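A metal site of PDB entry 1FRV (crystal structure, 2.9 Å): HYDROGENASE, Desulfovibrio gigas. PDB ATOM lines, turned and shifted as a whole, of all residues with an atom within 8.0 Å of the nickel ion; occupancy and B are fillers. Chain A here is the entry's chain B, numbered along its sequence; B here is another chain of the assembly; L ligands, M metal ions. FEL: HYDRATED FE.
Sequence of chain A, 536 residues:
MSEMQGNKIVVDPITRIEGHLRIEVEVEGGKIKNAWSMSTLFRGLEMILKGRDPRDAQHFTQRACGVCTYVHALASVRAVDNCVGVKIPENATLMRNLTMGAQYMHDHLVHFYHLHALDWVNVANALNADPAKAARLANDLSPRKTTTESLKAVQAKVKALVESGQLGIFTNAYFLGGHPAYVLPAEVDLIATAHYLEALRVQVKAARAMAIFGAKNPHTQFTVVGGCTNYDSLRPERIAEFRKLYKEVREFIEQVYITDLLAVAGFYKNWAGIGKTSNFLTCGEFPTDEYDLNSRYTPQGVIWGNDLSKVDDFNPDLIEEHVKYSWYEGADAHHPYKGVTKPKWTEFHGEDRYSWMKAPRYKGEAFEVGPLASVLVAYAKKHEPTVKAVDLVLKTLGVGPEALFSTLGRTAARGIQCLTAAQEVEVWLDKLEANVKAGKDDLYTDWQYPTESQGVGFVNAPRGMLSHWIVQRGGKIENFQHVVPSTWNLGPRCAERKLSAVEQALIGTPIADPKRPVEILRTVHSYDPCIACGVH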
ATOM      1  N   GLU A  18      28.580  15.964  -1.897  1.00  0.00           N
ATOM      2  CA  GLU A  18      28.581  16.073  -0.444  1.00  0.00           C
ATOM      3  C   GLU A  18      28.620  14.618   0.042  1.00  0.00           C
ATOM      4  O   GLU A  18      27.787  13.799  -0.359  1.00  0.00           O
ATOM      5  CB  GLU A  18      27.408  16.762   0.180  1.00  0.00           C
ATOM      6  CG  GLU A  18      27.338  16.924   1.695  1.00  0.00           C
ATOM      7  CD  GLU A  18      27.245  15.705   2.526  1.00  0.00           C
ATOM      8  OE1 GLU A  18      26.642  14.690   2.227  1.00  0.00           O
ATOM      9  OE2 GLU A  18      27.839  15.784   3.630  1.00  0.00           O
ATOM     10  N   GLN A  62      19.156  17.736  12.055  1.00  0.00           N
ATOM     11  CA  GLN A  62      19.471  18.909  11.192  1.00  0.00           C
ATOM     12  C   GLN A  62      20.933  18.763  10.769  1.00  0.00           C
ATOM     13  O   GLN A  62      21.374  19.262   9.732  1.00  0.00           O
ATOM     14  CB  GLN A  62      19.193  20.282  11.786  1.00  0.00           C
ATOM     15  CG  GLN A  62      18.861  21.297  10.687  1.00  0.00           C
ATOM     16  CD  GLN A  62      19.110  22.728  11.061  1.00  0.00           C
ATOM     17  OE1 GLN A  62      19.226  23.621  10.228  1.00  0.00           O
ATOM     18  NE2 GLN A  62      19.227  22.963  12.365  1.00  0.00           N
ATOM     19  N   ALA A  64      22.242  16.072   9.908  1.00  0.00           N
ATOM     20  CA  ALA A  64      22.326  14.958   8.942  1.00  0.00           C
ATOM     21  C   ALA A  64      23.319  15.564   7.922  1.00  0.00           C
ATOM     22  O   ALA A  64      24.297  14.920   7.578  1.00  0.00           O
ATOM     23  CB  ALA A  64      21.045  14.536   8.294  1.00  0.00           C
ATOM     24  N   CYS A  65      23.015  16.817   7.597  1.00  0.00           N
ATOM     25  CA  CYS A  65      23.955  17.517   6.663  1.00  0.00           C
ATOM     26  C   CYS A  65      23.725  19.013   6.655  1.00  0.00           C
ATOM     27  O   CYS A  65      22.786  19.487   7.290  1.00  0.00           O
ATOM     28  CB  CYS A  65      24.068  16.748   5.412  1.00  0.00           C
ATOM     29  SG  CYS A  65      23.291  17.259   3.915  1.00  0.00           S
ATOM     30  N   GLY A  66      24.620  19.755   6.045  1.00  0.00           N
ATOM     31  CA  GLY A  66      24.654  21.190   5.992  1.00  0.00           C
ATOM     32  C   GLY A  66      24.590  21.833   4.633  1.00  0.00           C
ATOM     33  O   GLY A  66      24.433  23.081   4.531  1.00  0.00           O
ATOM     34  N   VAL A  67      24.729  20.990   3.600  1.00  0.00           N
ATOM     35  CA  VAL A  67      24.601  21.558   2.235  1.00  0.00           C
ATOM     36  C   VAL A  67      23.085  21.891   2.211  1.00  0.00           C
ATOM     37  O   VAL A  67      22.726  23.058   2.101  1.00  0.00           O
ATOM     38  CB  VAL A  67      25.058  20.646   1.127  1.00  0.00           C
ATOM     39  CG1 VAL A  67      26.572  20.609   0.955  1.00  0.00           C
ATOM     40  CG2 VAL A  67      24.476  19.247   1.294  1.00  0.00           C
ATOM     41  N   CYS A  68      22.330  20.813   2.391  1.00  0.00           N
ATOM     42  CA  CYS A  68      20.868  20.896   2.451  1.00  0.00           C
ATOM     43  C   CYS A  68      20.450  21.217   3.885  1.00  0.00           C
ATOM     44  O   CYS A  68      19.731  20.449   4.527  1.00  0.00           O
ATOM     45  CB  CYS A  68      20.194  19.640   1.962  1.00  0.00           C
ATOM     46  SG  CYS A  68      20.366  18.182   3.018  1.00  0.00           S
ATOM     47  N   THR A  69      20.942  22.368   4.332  1.00  0.00           N
ATOM     48  CA  THR A  69      20.653  22.860   5.676  1.00  0.00           C
ATOM     49  C   THR A  69      19.136  23.015   5.809  1.00  0.00           C
ATOM     50  O   THR A  69      18.388  23.014   4.824  1.00  0.00           O
ATOM     51  CB  THR A  69      21.429  24.167   6.058  1.00  0.00           C
ATOM     52  OG1 THR A  69      21.529  24.196   7.522  1.00  0.00           O
ATOM     53  CG2 THR A  69      20.813  25.466   5.554  1.00  0.00           C
ATOM     54  N   VAL A  71      16.293  21.691   5.948  1.00  0.00           N
ATOM     55  CA  VAL A  71      15.372  20.640   5.562  1.00  0.00           C
ATOM     56  C   VAL A  71      15.166  19.474   6.514  1.00  0.00           C
ATOM     57  O   VAL A  71      14.059  18.871   6.522  1.00  0.00           O
ATOM     58  CB  VAL A  71      15.474  20.157   4.095  1.00  0.00           C
ATOM     59  CG1 VAL A  71      16.066  21.139   3.112  1.00  0.00           C
ATOM     60  CG2 VAL A  71      16.133  18.787   3.972  1.00  0.00           C
ATOM     61  N   HIS A  72      16.161  19.098   7.275  1.00  0.00           N
ATOM     62  CA  HIS A  72      16.044  17.963   8.221  1.00  0.00           C
ATOM     63  C   HIS A  72      15.468  18.512   9.533  1.00  0.00           C
ATOM     64  O   HIS A  72      14.973  17.737  10.361  1.00  0.00           O
ATOM     65  CB  HIS A  72      17.309  17.157   8.428  1.00  0.00           C
ATOM     66  CG  HIS A  72      17.747  16.183   7.397  1.00  0.00           C
ATOM     67  ND1 HIS A  72      17.127  14.999   7.099  1.00  0.00           N
ATOM     68  CD2 HIS A  72      18.842  16.222   6.578  1.00  0.00           C
ATOM     69  CE1 HIS A  72      17.786  14.363   6.146  1.00  0.00           C
ATOM     70  NE2 HIS A  72      18.849  15.084   5.824  1.00  0.00           N
ATOM     71  N   GLN A 103      16.129  27.828   0.449  1.00  0.00           N
ATOM     72  CA  GLN A 103      16.965  26.617   0.491  1.00  0.00           C
ATOM     73  C   GLN A 103      17.073  26.123  -0.968  1.00  0.00           C
ATOM     74  O   GLN A 103      18.132  25.663  -1.423  1.00  0.00           O
ATOM     75  CB  GLN A 103      16.418  25.532   1.397  1.00  0.00           C
ATOM     76  CG  GLN A 103      17.373  24.538   1.970  1.00  0.00           C
ATOM     77  CD  GLN A 103      18.821  24.925   1.963  1.00  0.00           C
ATOM     78  OE1 GLN A 103      19.323  25.777   2.698  1.00  0.00           O
ATOM     79  NE2 GLN A 103      19.559  24.285   1.058  1.00  0.00           N
ATOM     80  N   ASP A 107      20.642  26.347  -2.661  1.00  0.00           N
ATOM     81  CA  ASP A 107      21.063  24.969  -2.925  1.00  0.00           C
ATOM     82  C   ASP A 107      21.336  24.770  -4.407  1.00  0.00           C
ATOM     83  O   ASP A 107      22.495  24.430  -4.748  1.00  0.00           O
ATOM     84  CB  ASP A 107      20.142  23.971  -2.264  1.00  0.00           C
ATOM     85  CG  ASP A 107      20.768  22.650  -1.886  1.00  0.00           C
ATOM     86  OD1 ASP A 107      21.768  22.287  -2.554  1.00  0.00           O
ATOM     87  OD2 ASP A 107      20.310  21.949  -0.981  1.00  0.00           O
ATOM     88  N   ALA A 461      12.653  17.983  -0.075  1.00  0.00           N
ATOM     89  CA  ALA A 461      13.952  18.642  -0.037  1.00  0.00           C
ATOM     90  C   ALA A 461      14.444  18.890  -1.451  1.00  0.00           C
ATOM     91  O   ALA A 461      13.969  18.210  -2.372  1.00  0.00           O
ATOM     92  CB  ALA A 461      14.900  17.792   0.794  1.00  0.00           C
ATOM     93  N   PRO A 462      15.370  19.824  -1.582  1.00  0.00           N
ATOM     94  CA  PRO A 462      15.962  20.184  -2.867  1.00  0.00           C
ATOM     95  C   PRO A 462      16.491  19.027  -3.707  1.00  0.00           C
ATOM     96  O   PRO A 462      16.895  19.194  -4.884  1.00  0.00           O
ATOM     97  CB  PRO A 462      17.094  21.151  -2.502  1.00  0.00           C
ATOM     98  CG  PRO A 462      16.752  21.681  -1.131  1.00  0.00           C
ATOM     99  CD  PRO A 462      15.924  20.605  -0.452  1.00  0.00           C
ATOM    100  N   ARG A 463      16.510  17.846  -3.123  1.00  0.00           N
ATOM    101  CA  ARG A 463      16.967  16.629  -3.800  1.00  0.00           C
ATOM    102  C   ARG A 463      15.870  15.565  -3.739  1.00  0.00           C
ATOM    103  O   ARG A 463      16.133  14.408  -4.081  1.00  0.00           O
ATOM    104  CB  ARG A 463      18.254  16.027  -3.206  1.00  0.00           C
ATOM    105  CG  ARG A 463      19.553  16.650  -3.677  1.00  0.00           C
ATOM    106  CD  ARG A 463      20.510  16.795  -2.547  1.00  0.00           C
ATOM    107  NE  ARG A 463      21.494  17.827  -2.752  1.00  0.00           N
ATOM    108  CZ  ARG A 463      21.489  19.037  -2.202  1.00  0.00           C
ATOM    109  NH1 ARG A 463      20.506  19.460  -1.405  1.00  0.00           N
ATOM    110  NH2 ARG A 463      22.520  19.848  -2.460  1.00  0.00           N
ATOM    111  N   VAL A 484      15.839   9.378   3.474  1.00  0.00           N
ATOM    112  CA  VAL A 484      16.193  10.621   2.760  1.00  0.00           C
ATOM    113  C   VAL A 484      16.393  10.398   1.268  1.00  0.00           C
ATOM    114  O   VAL A 484      16.923   9.352   0.894  1.00  0.00           O
ATOM    115  CB  VAL A 484      17.496  11.183   3.417  1.00  0.00           C
ATOM    116  CG1 VAL A 484      17.627  12.689   3.248  1.00  0.00           C
ATOM    117  CG2 VAL A 484      17.656  10.770   4.853  1.00  0.00           C
ATOM    118  N   PRO A 485      16.022  11.383   0.471  1.00  0.00           N
ATOM    119  CA  PRO A 485      16.103  11.377  -0.980  1.00  0.00           C
ATOM    120  C   PRO A 485      17.204  10.528  -1.559  1.00  0.00           C
ATOM    121  O   PRO A 485      16.950   9.533  -2.254  1.00  0.00           O
ATOM    122  CB  PRO A 485      16.305  12.860  -1.326  1.00  0.00           C
ATOM    123  CG  PRO A 485      15.529  13.587  -0.278  1.00  0.00           C
ATOM    124  CD  PRO A 485      15.403  12.656   0.913  1.00  0.00           C
ATOM    125  N   SER A 486      18.436  10.964  -1.266  1.00  0.00           N
ATOM    126  CA  SER A 486      19.651  10.304  -1.744  1.00  0.00           C
ATOM    127  C   SER A 486      19.656   8.833  -1.370  1.00  0.00           C
ATOM    128  O   SER A 486      20.380   8.067  -2.015  1.00  0.00           O
ATOM    129  CB  SER A 486      20.907  11.013  -1.297  1.00  0.00           C
ATOM    130  OG  SER A 486      21.049  12.250  -1.976  1.00  0.00           O
ATOM    131  N   ASP A 528      22.743  15.113  -7.791  1.00  0.00           N
ATOM    132  CA  ASP A 528      23.193  15.831  -6.582  1.00  0.00           C
ATOM    133  C   ASP A 528      23.286  14.890  -5.375  1.00  0.00           C
ATOM    134  O   ASP A 528      22.485  15.055  -4.427  1.00  0.00           O
ATOM    135  CB  ASP A 528      22.106  16.898  -6.376  1.00  0.00           C
ATOM    136  CG  ASP A 528      22.478  18.136  -5.642  1.00  0.00           C
ATOM    137  OD1 ASP A 528      23.411  18.105  -4.824  1.00  0.00           O
ATOM    138  OD2 ASP A 528      21.886  19.195  -5.871  1.00  0.00           O
ATOM    139  N   PRO A 529      24.234  13.954  -5.402  1.00  0.00           N
ATOM    140  CA  PRO A 529      24.383  12.964  -4.328  1.00  0.00           C
ATOM    141  C   PRO A 529      24.819  13.600  -3.033  1.00  0.00           C
ATOM    142  O   PRO A 529      25.732  14.446  -3.034  1.00  0.00           O
ATOM    143  CB  PRO A 529      25.294  11.923  -4.899  1.00  0.00           C
ATOM    144  CG  PRO A 529      25.865  12.428  -6.174  1.00  0.00           C
ATOM    145  CD  PRO A 529      25.183  13.740  -6.493  1.00  0.00           C
ATOM    146  N   CYS A 530      24.164  13.218  -1.957  1.00  0.00           N
ATOM    147  CA  CYS A 530      24.418  13.727  -0.589  1.00  0.00           C
ATOM    148  C   CYS A 530      24.413  12.575   0.412  1.00  0.00           C
ATOM    149  O   CYS A 530      23.450  12.251   1.116  1.00  0.00           O
ATOM    150  CB  CYS A 530      23.305  14.732  -0.313  1.00  0.00           C
ATOM    151  SG  CYS A 530      23.808  15.968   0.878  1.00  0.00           S
ATOM    152  N   ILE A 531      25.540  11.902   0.477  1.00  0.00           N
ATOM    153  CA  ILE A 531      25.841  10.730   1.257  1.00  0.00           C
ATOM    154  C   ILE A 531      25.764  10.830   2.749  1.00  0.00           C
ATOM    155  O   ILE A 531      25.606   9.774   3.405  1.00  0.00           O
ATOM    156  CB  ILE A 531      27.209  10.102   0.750  1.00  0.00           C
ATOM    157  CG1 ILE A 531      27.324  10.379  -0.776  1.00  0.00           C
ATOM    158  CG2 ILE A 531      27.280   8.591   1.083  1.00  0.00           C
ATOM    159  CD1 ILE A 531      26.202   9.681  -1.611  1.00  0.00           C
ATOM    160  N   ALA A 532      25.886  12.034   3.267  1.00  0.00           N
ATOM    161  CA  ALA A 532      25.811  12.302   4.716  1.00  0.00           C
ATOM    162  C   ALA A 532      24.343  12.176   5.142  1.00  0.00           C
ATOM    163  O   ALA A 532      24.023  11.669   6.225  1.00  0.00           O
ATOM    164  CB  ALA A 532      26.386  13.664   5.036  1.00  0.00           C
ATOM    165  N   CYS A 533      23.474  12.629   4.250  1.00  0.00           N
ATOM    166  CA  CYS A 533      22.026  12.565   4.378  1.00  0.00           C
ATOM    167  C   CYS A 533      21.690  11.039   4.314  1.00  0.00           C
ATOM    168  O   CYS A 533      21.346  10.394   5.289  1.00  0.00           O
ATOM    169  CB  CYS A 533      21.254  13.187   3.227  1.00  0.00           C
ATOM    170  SG  CYS A 533      20.994  14.945   3.184  1.00  0.00           S
ATOM    171  N   GLY A 534      21.836  10.592   3.077  1.00  0.00           N
ATOM    172  CA  GLY A 534      21.581   9.254   2.610  1.00  0.00           C
ATOM    173  C   GLY A 534      21.748   8.169   3.649  1.00  0.00           C
ATOM    174  O   GLY A 534      20.821   7.400   3.929  1.00  0.00           O
ATOM    175  N   CYS B  17      29.447  16.714   7.980  1.00  0.00           N
ATOM    176  CA  CYS B  17      28.086  16.864   7.442  1.00  0.00           C
ATOM    177  C   CYS B  17      28.031  18.055   6.475  1.00  0.00           C
ATOM    178  O   CYS B  17      26.971  18.488   6.045  1.00  0.00           O
ATOM    179  CB  CYS B  17      27.075  17.097   8.568  1.00  0.00           C
ATOM    180  SG  CYS B  17      26.730  18.830   8.935  1.00  0.00           S
ATOM    181  N   THR B  18      29.210  18.579   6.216  1.00  0.00           N
ATOM    182  CA  THR B  18      29.506  19.705   5.372  1.00  0.00           C
ATOM    183  C   THR B  18      28.974  21.059   5.812  1.00  0.00           C
ATOM    184  O   THR B  18      28.964  22.029   5.026  1.00  0.00           O
ATOM    185  CB  THR B  18      29.214  19.407   3.844  1.00  0.00           C
ATOM    186  OG1 THR B  18      29.077  17.953   3.789  1.00  0.00           O
ATOM    187  CG2 THR B  18      30.390  19.897   2.978  1.00  0.00           C
HETATM  188 FE   FEL L   1      19.743  16.035   1.646  1.00  0.00          FE
HETATM  189  O1  FEL L   1      19.704  14.196   0.782  1.00  0.00           O
HETATM  190  O2  FEL L   1      18.612  17.490   0.946  1.00  0.00           O
HETATM  191  O3  FEL L   1      18.056  15.561   2.456  1.00  0.00           O
HETATM  192 NI    NI M   1      22.141  17.086   2.248  1.00  0.00          NI
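Merely in contact with the nickel ion: Val 67 (3.3 Å).
Five residues have an atom within 4 Å of the nickel ion: Cys 65, Val 67, Cys 68, Cys 530 and Cys 533.
The side-chain sulfur (SG) of Cys 68 is bound to an iron atom (FE) of the ligand (2.6 Å).
The side-chain sulfur of Cys 533 is bound to an iron atom (FE) of the ligand.
The nickel ion is bound by SG of Cys 65, 2.0 Å away.
The nickel ion is bound by SG of Cys 68, 2.2 Å away.
The side-chain sulfur (SG) of Cys 530 binds the nickel ion.
The side-chain sulfur (SG) of Cys 533 is bound to the nickel ion (2.6 Å).
SG of Cys 530 lies close to OE1 of Glu 18 of chain A (3.4 Å).
The backbone NH (N) of Cys 530 is in hydrogen-bond range of the side-chain hydroxyl (OG) of Ser 486 (3.3 Å).
The side-chain sulfur of Cys 533 sits close to a ring nitrogen (NE2) of His 72 (3.4 Å).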
